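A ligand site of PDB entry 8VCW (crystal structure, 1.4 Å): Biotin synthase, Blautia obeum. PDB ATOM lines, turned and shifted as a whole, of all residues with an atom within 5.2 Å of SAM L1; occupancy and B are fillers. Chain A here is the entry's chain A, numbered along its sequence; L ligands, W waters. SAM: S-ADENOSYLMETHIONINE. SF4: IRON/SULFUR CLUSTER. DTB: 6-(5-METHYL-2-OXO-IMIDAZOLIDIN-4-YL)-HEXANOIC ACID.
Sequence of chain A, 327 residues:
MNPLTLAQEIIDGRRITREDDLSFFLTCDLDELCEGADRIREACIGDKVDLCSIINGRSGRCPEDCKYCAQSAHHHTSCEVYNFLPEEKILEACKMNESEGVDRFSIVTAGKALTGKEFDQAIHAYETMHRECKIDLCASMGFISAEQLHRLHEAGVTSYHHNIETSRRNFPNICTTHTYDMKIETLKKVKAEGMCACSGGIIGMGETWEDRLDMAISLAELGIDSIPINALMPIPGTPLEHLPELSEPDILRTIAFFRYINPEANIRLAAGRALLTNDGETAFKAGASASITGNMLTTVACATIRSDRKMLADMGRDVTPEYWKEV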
ATOM      1  N   TYR A  68      15.546  33.592  -5.340  1.00  0.00           N
ATOM      2  CA  TYR A  68      16.377  33.121  -4.241  1.00  0.00           C
ATOM      3  C   TYR A  68      17.864  33.230  -4.515  1.00  0.00           C
ATOM      4  O   TYR A  68      18.671  33.048  -3.575  1.00  0.00           O
ATOM      5  CB  TYR A  68      16.047  31.627  -3.941  1.00  0.00           C
ATOM      6  CG  TYR A  68      16.085  30.747  -5.177  1.00  0.00           C
ATOM      7  CD1 TYR A  68      17.296  30.321  -5.700  1.00  0.00           C
ATOM      8  CD2 TYR A  68      14.907  30.416  -5.892  1.00  0.00           C
ATOM      9  CE1 TYR A  68      17.367  29.569  -6.846  1.00  0.00           C
ATOM     10  CE2 TYR A  68      15.009  29.662  -7.056  1.00  0.00           C
ATOM     11  CZ  TYR A  68      16.220  29.271  -7.521  1.00  0.00           C
ATOM     12  OH  TYR A  68      16.276  28.509  -8.704  1.00  0.00           O
ATOM     13  N   CYS A  69      18.258  33.472  -5.773  1.00  0.00           N
ATOM     14  CA  CYS A  69      19.597  33.091  -6.191  1.00  0.00           C
ATOM     15  C   CYS A  69      20.599  34.252  -6.073  1.00  0.00           C
ATOM     16  O   CYS A  69      20.433  35.311  -6.684  1.00  0.00           O
ATOM     17  CB  CYS A  69      19.562  32.610  -7.629  1.00  0.00           C
ATOM     18  SG  CYS A  69      21.203  31.940  -8.138  1.00  0.00           S
ATOM     19  N   ALA A  70      21.704  34.004  -5.370  1.00  0.00           N
ATOM     20  CA  ALA A  70      22.776  34.971  -5.252  1.00  0.00           C
ATOM     21  C   ALA A  70      23.424  35.286  -6.603  1.00  0.00           C
ATOM     22  O   ALA A  70      24.074  36.350  -6.707  1.00  0.00           O
ATOM     23  CB  ALA A  70      23.843  34.436  -4.304  1.00  0.00           C
ATOM     24  N   VAL A 108      29.000  22.907 -11.140  1.00  0.00           N
ATOM     25  CA  VAL A 108      27.734  23.646 -11.145  1.00  0.00           C
ATOM     26  C   VAL A 108      27.969  25.031 -11.729  1.00  0.00           C
ATOM     27  O   VAL A 108      28.834  25.756 -11.234  1.00  0.00           O
ATOM     28  CB  VAL A 108      27.235  23.812  -9.711  1.00  0.00           C
ATOM     29  CG1 VAL A 108      25.897  24.548  -9.709  1.00  0.00           C
ATOM     30  CG2 VAL A 108      27.102  22.459  -9.051  1.00  0.00           C
ATOM     31  N   THR A 109      27.209  25.407 -12.740  1.00  0.00           N
ATOM     32  CA  THR A 109      27.454  26.661 -13.427  1.00  0.00           C
ATOM     33  C   THR A 109      26.264  27.594 -13.340  1.00  0.00           C
ATOM     34  O   THR A 109      25.144  27.177 -13.563  1.00  0.00           O
ATOM     35  CB  THR A 109      27.882  26.453 -14.885  1.00  0.00           C
ATOM     36  OG1 THR A 109      26.857  25.712 -15.585  1.00  0.00           O
ATOM     37  CG2 THR A 109      29.228  25.711 -14.940  1.00  0.00           C
ATOM     38  N   ALA A 110      26.523  28.860 -13.056  1.00  0.00           N
ATOM     39  CA  ALA A 110      25.482  29.876 -13.171  1.00  0.00           C
ATOM     40  C   ALA A 110      25.193  30.125 -14.635  1.00  0.00           C
ATOM     41  O   ALA A 110      26.040  29.914 -15.506  1.00  0.00           O
ATOM     42  CB  ALA A 110      25.987  31.183 -12.556  1.00  0.00           C
ATOM     43  N   GLY A 111      23.970  30.559 -14.940  1.00  0.00           N
ATOM     44  CA  GLY A 111      23.599  30.851 -16.313  1.00  0.00           C
ATOM     45  C   GLY A 111      22.395  30.046 -16.737  1.00  0.00           C
ATOM     46  O   GLY A 111      22.052  29.056 -16.097  1.00  0.00           O
ATOM     47  N   SER A 140      25.657  20.169 -13.164  1.00  0.00           N
ATOM     48  CA  SER A 140      24.472  21.028 -13.013  1.00  0.00           C
ATOM     49  C   SER A 140      24.701  22.265 -13.862  1.00  0.00           C
ATOM     50  O   SER A 140      25.427  23.184 -13.454  1.00  0.00           O
ATOM     51  CB  SER A 140      24.318  21.393 -11.551  1.00  0.00           C
ATOM     52  OG  SER A 140      23.096  22.110 -11.377  1.00  0.00           O
ATOM     53  N   MET A 141      24.067  22.308 -15.014  1.00  0.00           N
ATOM     54  CA  MET A 141      24.435  23.271 -16.056  1.00  0.00           C
ATOM     55  C   MET A 141      23.247  23.978 -16.676  1.00  0.00           C
ATOM     56  O   MET A 141      23.430  24.719 -17.638  1.00  0.00           O
ATOM     57  CB  MET A 141      25.301  22.583 -17.117  1.00  0.00           C
ATOM     58  CG  MET A 141      26.604  22.180 -16.581  1.00  0.00           C
ATOM     59  SD  MET A 141      27.464  21.196 -17.773  1.00  0.00           S
ATOM     60  CE  MET A 141      28.964  20.833 -16.951  1.00  0.00           C
ATOM     61  N   GLY A 142      22.074  23.845 -16.115  1.00  0.00           N
ATOM     62  CA  GLY A 142      20.927  24.513 -16.660  1.00  0.00           C
ATOM     63  C   GLY A 142      20.278  23.764 -17.819  1.00  0.00           C
ATOM     64  O   GLY A 142      20.272  22.544 -17.895  1.00  0.00           O
ATOM     65  N   HIS A 161      21.982  17.208 -12.605  1.00  0.00           N
ATOM     66  CA  HIS A 161      21.188  17.899 -11.603  1.00  0.00           C
ATOM     67  C   HIS A 161      20.358  18.988 -12.264  1.00  0.00           C
ATOM     68  O   HIS A 161      20.880  19.845 -13.006  1.00  0.00           O
ATOM     69  CB  HIS A 161      22.161  18.566 -10.637  1.00  0.00           C
ATOM     70  CG  HIS A 161      21.485  19.356  -9.568  1.00  0.00           C
ATOM     71  ND1 HIS A 161      21.431  20.741  -9.572  1.00  0.00           N
ATOM     72  CD2 HIS A 161      20.832  18.941  -8.457  1.00  0.00           C
ATOM     73  CE1 HIS A 161      20.752  21.124  -8.484  1.00  0.00           C
ATOM     74  NE2 HIS A 161      20.418  20.068  -7.787  1.00  0.00           N
ATOM     75  N   HIS A 162      19.074  19.028 -11.951  1.00  0.00           N
ATOM     76  CA  HIS A 162      18.208  20.091 -12.498  1.00  0.00           C
ATOM     77  C   HIS A 162      16.990  20.177 -11.576  1.00  0.00           C
ATOM     78  O   HIS A 162      16.068  19.369 -11.705  1.00  0.00           O
ATOM     79  CB  HIS A 162      17.793  19.678 -13.922  1.00  0.00           C
ATOM     80  CG  HIS A 162      17.231  20.767 -14.774  1.00  0.00           C
ATOM     81  ND1 HIS A 162      17.983  21.800 -15.261  1.00  0.00           N
ATOM     82  CD2 HIS A 162      16.002  20.881 -15.339  1.00  0.00           C
ATOM     83  CE1 HIS A 162      17.214  22.548 -16.056  1.00  0.00           C
ATOM     84  NE2 HIS A 162      16.008  21.994 -16.125  1.00  0.00           N
ATOM     85  N   ASN A 163      17.022  21.083 -10.604  1.00  0.00           N
ATOM     86  CA  ASN A 163      15.959  21.174  -9.612  1.00  0.00           C
ATOM     87  C   ASN A 163      14.696  21.773 -10.203  1.00  0.00           C
ATOM     88  O   ASN A 163      14.730  22.684 -11.038  1.00  0.00           O
ATOM     89  CB  ASN A 163      16.437  22.105  -8.487  1.00  0.00           C
ATOM     90  CG  ASN A 163      17.339  21.395  -7.508  1.00  0.00           C
ATOM     91  OD1 ASN A 163      17.392  20.176  -7.452  1.00  0.00           O
ATOM     92  ND2 ASN A 163      18.028  22.160  -6.707  1.00  0.00           N
ATOM     93  N   GLU A 165      12.769  23.280  -8.125  1.00  0.00           N
ATOM     94  CA  GLU A 165      12.782  24.483  -7.267  1.00  0.00           C
ATOM     95  C   GLU A 165      11.569  24.588  -6.371  1.00  0.00           C
ATOM     96  O   GLU A 165      11.689  24.758  -5.151  1.00  0.00           O
ATOM     97  CB  GLU A 165      13.110  25.813  -7.968  1.00  0.00           C
ATOM     98  CG  GLU A 165      14.262  25.684  -8.943  1.00  0.00           C
ATOM     99  CD  GLU A 165      15.609  25.466  -8.275  1.00  0.00           C
ATOM    100  OE1 GLU A 165      15.684  25.225  -7.047  1.00  0.00           O
ATOM    101  OE2 GLU A 165      16.611  25.419  -9.047  1.00  0.00           O
ATOM    102  N   LYS A 183      11.749  22.857 -16.992  1.00  0.00           N
ATOM    103  CA  LYS A 183      12.499  21.971 -16.108  1.00  0.00           C
ATOM    104  C   LYS A 183      12.126  20.522 -16.376  1.00  0.00           C
ATOM    105  O   LYS A 183      12.984  19.628 -16.476  1.00  0.00           O
ATOM    106  CB  LYS A 183      12.152  22.305 -14.653  1.00  0.00           C
ATOM    107  CG  LYS A 183      12.606  23.674 -14.157  1.00  0.00           C
ATOM    108  CD  LYS A 183      14.122  23.722 -13.974  1.00  0.00           C
ATOM    109  CE  LYS A 183      14.539  24.984 -13.162  1.00  0.00           C
ATOM    110  NZ  LYS A 183      15.934  24.706 -12.725  1.00  0.00           N
ATOM    111  N   GLY A 201      14.462  20.815  -4.771  1.00  0.00           N
ATOM    112  CA  GLY A 201      14.136  22.226  -4.805  1.00  0.00           C
ATOM    113  C   GLY A 201      14.432  22.845  -3.460  1.00  0.00           C
ATOM    114  O   GLY A 201      15.280  22.351  -2.711  1.00  0.00           O
ATOM    115  N   ILE A 202      13.744  23.962  -3.213  1.00  0.00           N
ATOM    116  CA  ILE A 202      14.003  24.824  -2.057  1.00  0.00           C
ATOM    117  C   ILE A 202      12.707  24.987  -1.299  1.00  0.00           C
ATOM    118  O   ILE A 202      11.696  25.401  -1.866  1.00  0.00           O
ATOM    119  CB  ILE A 202      14.576  26.208  -2.460  1.00  0.00           C
ATOM    120  CG1 ILE A 202      15.808  26.090  -3.347  1.00  0.00           C
ATOM    121  CG2 ILE A 202      14.934  26.966  -1.179  1.00  0.00           C
ATOM    122  CD1 ILE A 202      16.187  27.440  -3.896  1.00  0.00           C
ATOM    123  N   ASN A 230      16.692  21.455  -0.322  1.00  0.00           N
ATOM    124  CA  ASN A 230      17.400  22.633   0.176  1.00  0.00           C
ATOM    125  C   ASN A 230      16.469  23.427   1.049  1.00  0.00           C
ATOM    126  O   ASN A 230      15.342  23.672   0.647  1.00  0.00           O
ATOM    127  CB  ASN A 230      17.794  23.570  -0.985  1.00  0.00           C
ATOM    128  CG  ASN A 230      18.779  22.930  -1.939  1.00  0.00           C
ATOM    129  OD1 ASN A 230      20.014  23.033  -1.756  1.00  0.00           O
ATOM    130  ND2 ASN A 230      18.282  22.250  -2.918  1.00  0.00           N
ATOM    131  N   ALA A 231      16.905  23.850   2.246  1.00  0.00           N
ATOM    132  CA  ALA A 231      16.163  24.868   2.959  1.00  0.00           C
ATOM    133  C   ALA A 231      16.710  26.224   2.523  1.00  0.00           C
ATOM    134  O   ALA A 231      17.922  26.358   2.300  1.00  0.00           O
ATOM    135  CB  ALA A 231      16.271  24.640   4.470  1.00  0.00           C
ATOM    136  N   LEU A 232      15.829  27.190   2.350  1.00  0.00           N
ATOM    137  CA  LEU A 232      16.265  28.492   1.857  1.00  0.00           C
ATOM    138  C   LEU A 232      17.358  29.069   2.760  1.00  0.00           C
ATOM    139  O   LEU A 232      17.194  29.141   3.975  1.00  0.00           O
ATOM    140  CB  LEU A 232      15.093  29.465   1.820  1.00  0.00           C
ATOM    141  CG  LEU A 232      15.473  30.862   1.296  1.00  0.00           C
ATOM    142  CD1 LEU A 232      15.937  30.896  -0.163  1.00  0.00           C
ATOM    143  CD2 LEU A 232      14.316  31.814   1.508  1.00  0.00           C
ATOM    144  N   MET A 233      18.429  29.492   2.115  1.00  0.00           N
ATOM    145  CA  MET A 233      19.426  30.349   2.741  1.00  0.00           C
ATOM    146  C   MET A 233      19.137  31.762   2.230  1.00  0.00           C
ATOM    147  O   MET A 233      19.467  32.082   1.099  1.00  0.00           O
ATOM    148  CB  MET A 233      20.825  29.893   2.315  1.00  0.00           C
ATOM    149  CG  MET A 233      21.090  28.496   2.883  1.00  0.00           C
ATOM    150  SD  MET A 233      22.759  27.889   2.465  1.00  0.00           S
ATOM    151  CE  MET A 233      23.745  28.732   3.702  1.00  0.00           C
ATOM    152  N   PRO A 234      18.513  32.621   2.996  1.00  0.00           N
ATOM    153  CA  PRO A 234      18.135  33.940   2.423  1.00  0.00           C
ATOM    154  C   PRO A 234      19.371  34.759   2.132  1.00  0.00           C
ATOM    155  O   PRO A 234      20.222  34.937   3.002  1.00  0.00           O
ATOM    156  CB  PRO A 234      17.254  34.575   3.509  1.00  0.00           C
ATOM    157  CG  PRO A 234      16.796  33.412   4.328  1.00  0.00           C
ATOM    158  CD  PRO A 234      17.936  32.424   4.329  1.00  0.00           C
ATOM    159  N   ILE A 235      19.512  35.208   0.890  1.00  0.00           N
ATOM    160  CA  ILE A 235      20.739  35.866   0.448  1.00  0.00           C
ATOM    161  C   ILE A 235      20.542  37.382   0.510  1.00  0.00           C
ATOM    162  O   ILE A 235      19.644  37.897  -0.155  1.00  0.00           O
ATOM    163  CB  ILE A 235      21.108  35.477  -0.978  1.00  0.00           C
ATOM    164  CG1 ILE A 235      21.242  33.943  -1.097  1.00  0.00           C
ATOM    165  CG2 ILE A 235      22.360  36.211  -1.414  1.00  0.00           C
ATOM    166  CD1 ILE A 235      22.369  33.348  -0.190  1.00  0.00           C
ATOM    167  N   ALA A 271      21.367  22.601   0.751  1.00  0.00           N
ATOM    168  CA  ALA A 271      21.592  23.868   1.418  1.00  0.00           C
ATOM    169  C   ALA A 271      20.766  23.972   2.686  1.00  0.00           C
ATOM    170  O   ALA A 271      19.704  23.366   2.830  1.00  0.00           O
ATOM    171  CB  ALA A 271      21.174  25.013   0.512  1.00  0.00           C
ATOM    172  N   LEU A 297      27.889  27.045  -3.090  1.00  0.00           N
ATOM    173  CA  LEU A 297      28.219  27.808  -4.297  1.00  0.00           C
ATOM    174  C   LEU A 297      28.718  29.195  -3.955  1.00  0.00           C
ATOM    175  O   LEU A 297      29.690  29.682  -4.575  1.00  0.00           O
ATOM    176  CB  LEU A 297      27.006  27.904  -5.225  1.00  0.00           C
ATOM    177  CG  LEU A 297      26.570  26.565  -5.775  1.00  0.00           C
ATOM    178  CD1 LEU A 297      25.302  26.780  -6.554  1.00  0.00           C
ATOM    179  CD2 LEU A 297      27.651  25.926  -6.645  1.00  0.00           C
HETATM  180  N   SAM L   1      21.899  27.587 -13.376  1.00  0.00           N
HETATM  181  CA  SAM L   1      21.643  26.143 -13.292  1.00  0.00           C
HETATM  182  C   SAM L   1      20.244  25.854 -12.791  1.00  0.00           C
HETATM  183  O   SAM L   1      19.570  26.781 -12.253  1.00  0.00           O
HETATM  184  OXT SAM L   1      19.804  24.698 -12.920  1.00  0.00           O
HETATM  185  CB  SAM L   1      22.733  25.483 -12.417  1.00  0.00           C
HETATM  186  CG  SAM L   1      22.867  25.999 -10.968  1.00  0.00           C
HETATM  187  SD  SAM L   1      21.470  25.681  -9.869  1.00  0.00           S
HETATM  188  CE  SAM L   1      21.702  23.915  -9.635  1.00  0.00           C
HETATM  189  C5' SAM L   1      21.934  26.016  -8.148  1.00  0.00           C
HETATM  190  C4' SAM L   1      20.917  25.400  -7.144  1.00  0.00           C
HETATM  191  O4' SAM L   1      21.155  26.002  -5.884  1.00  0.00           O
HETATM  192  C3' SAM L   1      19.513  25.802  -7.501  1.00  0.00           C
HETATM  193  O3' SAM L   1      18.976  24.722  -8.288  1.00  0.00           O
HETATM  194  C2' SAM L   1      18.819  26.014  -6.180  1.00  0.00           C
HETATM  195  O2' SAM L   1      17.960  24.947  -5.842  1.00  0.00           O
HETATM  196  C1' SAM L   1      19.958  26.037  -5.129  1.00  0.00           C
HETATM  197  N9  SAM L   1      20.033  27.373  -4.459  1.00  0.00           N
HETATM  198  C8  SAM L   1      20.431  28.526  -5.055  1.00  0.00           C
HETATM  199  N7  SAM L   1      20.262  29.514  -4.173  1.00  0.00           N
HETATM  200  C5  SAM L   1      19.811  29.000  -2.977  1.00  0.00           C
HETATM  201  C6  SAM L   1      19.505  29.531  -1.759  1.00  0.00           C
HETATM  202  N6  SAM L   1      19.627  30.864  -1.467  1.00  0.00           N
HETATM  203  N1  SAM L   1      19.049  28.745  -0.747  1.00  0.00           N
HETATM  204  C2  SAM L   1      18.887  27.408  -0.999  1.00  0.00           C
HETATM  205  N3  SAM L   1      19.176  26.840  -2.186  1.00  0.00           N
HETATM  206  C4  SAM L   1      19.641  27.635  -3.183  1.00  0.00           C
HETATM  207 FE1  SF4 L   2      20.466  31.487 -12.844  1.00  0.00          FE
HETATM  208 FE2  SF4 L   2      20.460  28.847 -11.955  1.00  0.00          FE
HETATM  209 FE3  SF4 L   2      18.290  30.686 -11.518  1.00  0.00          FE
HETATM  210 FE4  SF4 L   2      20.596  31.087 -10.200  1.00  0.00          FE
HETATM  211  S1  SF4 L   2      19.230  29.243  -9.964  1.00  0.00           S
HETATM  212  S2  SF4 L   2      19.394  32.709 -11.277  1.00  0.00           S
HETATM  213  S3  SF4 L   2      22.170  30.460 -11.691  1.00  0.00           S
HETATM  214  S4  SF4 L   2      18.978  29.869 -13.514  1.00  0.00           S
HETATM  215  CN  DTB L   3      21.299  21.500  -4.839  1.00  0.00           C
HETATM  216  O   DTB L   3      20.195  21.048  -4.962  1.00  0.00           O
HETATM  217  N2  DTB L   3      21.666  22.661  -4.109  1.00  0.00           N
HETATM  218  CR  DTB L   3      23.118  22.812  -4.151  1.00  0.00           C
HETATM  219  CS  DTB L   3      23.650  21.901  -5.195  1.00  0.00           C
HETATM  220  N1  DTB L   3      22.514  21.044  -5.463  1.00  0.00           N
HETATM  221  CT  DTB L   3      23.856  22.672  -6.525  1.00  0.00           C
HETATM  222  CE  DTB L   3      23.556  24.285  -4.169  1.00  0.00           C
HETATM  223  CD  DTB L   3      23.082  25.030  -2.914  1.00  0.00           C
HETATM  224  CG  DTB L   3      23.379  26.538  -3.047  1.00  0.00           C
HETATM  225  CB  DTB L   3      23.091  27.256  -1.709  1.00  0.00           C
HETATM  226  CA  DTB L   3      23.183  28.796  -1.863  1.00  0.00           C
HETATM  227  C   DTB L   3      24.572  29.320  -2.331  1.00  0.00           C
HETATM  228  OI1 DTB L   3      24.557  30.327  -3.125  1.00  0.00           O
HETATM  229  OI2 DTB L   3      25.648  28.792  -1.936  1.00  0.00           O
HETATM  230  O   HOH W   1      16.992  26.659 -11.210  1.00  0.00           O
HETATM  231  O   HOH W   2      19.178  27.427 -15.636  1.00  0.00           O
HETATM  232  O   HOH W   3      17.688  25.209 -14.755  1.00  0.00           O
HETATM  233  O   HOH W   4      20.649  22.309 -14.185  1.00  0.00           O
HETATM  234  O   HOH W   5      18.966  23.210 -10.820  1.00  0.00           O
HETATM  235  O   HOH W   6      24.176  28.399  -9.841  1.00  0.00           O
HETATM  236  O   HOH W   7      22.131  31.599  -3.865  1.00  0.00           O
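O of SAM L1 binds FE2 of SF4 L2 (2.3 Å).
Merely in contact with SAM L1: Ser 140 (2.9 Å), His 161 (3.2 Å), Ile 202 (3.5 Å), Ile 235 (3.5 Å), Val 108 (3.6 Å), Ala 231 (3.6 Å), Ala 271 (3.6 Å), Gly 142 (3.7 Å), Asn 230 (3.7 Å), Leu 297 (3.8 Å) and Leu 232 (3.8 Å).
Hydrophobic or aromatic side chains that line SAM L1: Tyr 68, Val 108, His 161, Ile 202, Leu 232, Met 233, Ile 235, Ala 271 and Leu 297.
Of the 25 residues printed, 18 come within 4 Å of SAM L1.
O of Glu 165 is in hydrogen-bond range of N of Ile 202 (2.9 Å).
The backbone carbonyl oxygen of Ser 140 is in hydrogen-bond range of the backbone NH of Thr 109 (2.9 Å).
A ring nitrogen (ND1) of His 161 is in hydrogen-bond range of the side-chain hydroxyl (OG) of Ser 140, at 2.8 Å.
The side-chain amide oxygen of Asn 163 lies within hydrogen-bond range of a ring nitrogen (NE2) of His 161 (3.0 Å).
The side-chain amino group (NZ) of Lys 183 lies within hydrogen-bond range of the backbone carbonyl oxygen (O) of Asn 163, 2.9 Å away.
The backbone NH (N) of Ala 231 sits at hydrogen-bond distance from the backbone carbonyl oxygen (O) of Ala 271 (2.9 Å).
The side-chain amide oxygen (OD1) of Asn 230 lies within hydrogen-bond range of the backbone NH (N) of Ala 271 (2.9 Å).
O of Gly 201 sits at hydrogen-bond distance from N of Asn 230 (2.9 Å).
Water W5 lies within hydrogen-bond range of OXT of SAM L1 (2.7 Å) and N of Asn 163 (2.9 Å).
Water W1 lies within hydrogen-bond range of OE2 of Glu 165 (2.5 Å), NZ of Lys 183 (2.7 Å), OH of Tyr 68 (3.2 Å) and S1 of SF4 L2 (3.6 Å).
Water W7 lies within hydrogen-bond range of a nitrogen (N7) of SAM L1 (2.8 Å), an oxygen (OI1) of DTB L3 (2.8 Å) and the backbone NH of Ala 70 (2.9 Å).
Water W4 lies within hydrogen-bond range of the backbone carbonyl oxygen of His 161 (2.7 Å), an oxygen (OXT) of SAM L1 (2.8 Å), the backbone NH of Gly 142 (2.8 Å) and a ring nitrogen (ND1) of His 162 (2.9 Å).
Water W3 lies within hydrogen-bond range of the side-chain amino group (NZ) of Lys 183 (2.7 Å), an oxygen (OXT) of SAM L1 (2.8 Å) and a ring nitrogen (ND1) of His 162 (3.5 Å).
Water W2 bridges S4 of SF4 L2 (3.2 Å) and O of Gly 111 (3.3 Å).
OE2 of Glu 165 sits at hydrogen-bond distance from O3' of SAM L1 (2.6 Å).
N1 of SAM L1 lies within hydrogen-bond range of N of Met 233 (3.0 Å).
A nitrogen (N6) of SAM L1 lies within hydrogen-bond range of the backbone carbonyl oxygen (O) of Met 233 (2.8 Å).
O2' of SAM L1 is in hydrogen-bond range of ND2 of Asn 163 (2.9 Å).
The backbone carbonyl oxygen (O) of Gly 111 lies close to a nitrogen (N) of SAM L1.
A nitrogen (N) of SAM L1 lies close to the backbone carbonyl oxygen (O) of Thr 109, 3.3 Å away.
The backbone carbonyl oxygen (O) of Tyr 68 sits at hydrogen-bond distance from a nitrogen (N6) of SAM L1.
OXT of SAM L1 lies within salt-bridge range of NZ of Lys 183, 3.9 Å away.
The backbone NH (N) of Gly 111 lies close to a sulfur (S3) of SF4 L2 (3.7 Å).
S1 of SF4 L2 lies close to OH of Tyr 68 (3.3 Å).
FE4 of SF4 L2 is bound by SG of Cys 69, at 2.3 Å.
The side-chain amide nitrogen (ND2) of Asn 163 sits at hydrogen-bond distance from an oxygen (O) of DTB L3 (3.0 Å).
NE2 of His 161 is in hydrogen-bond range of O of DTB L3 (3.0 Å).
The side-chain amide oxygen (OD1) of Asn 230 sits at hydrogen-bond distance from a nitrogen (N2) of DTB L3.
OI2 of DTB L3 sits at hydrogen-bond distance from N of Leu 297, at 3.1 Å.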
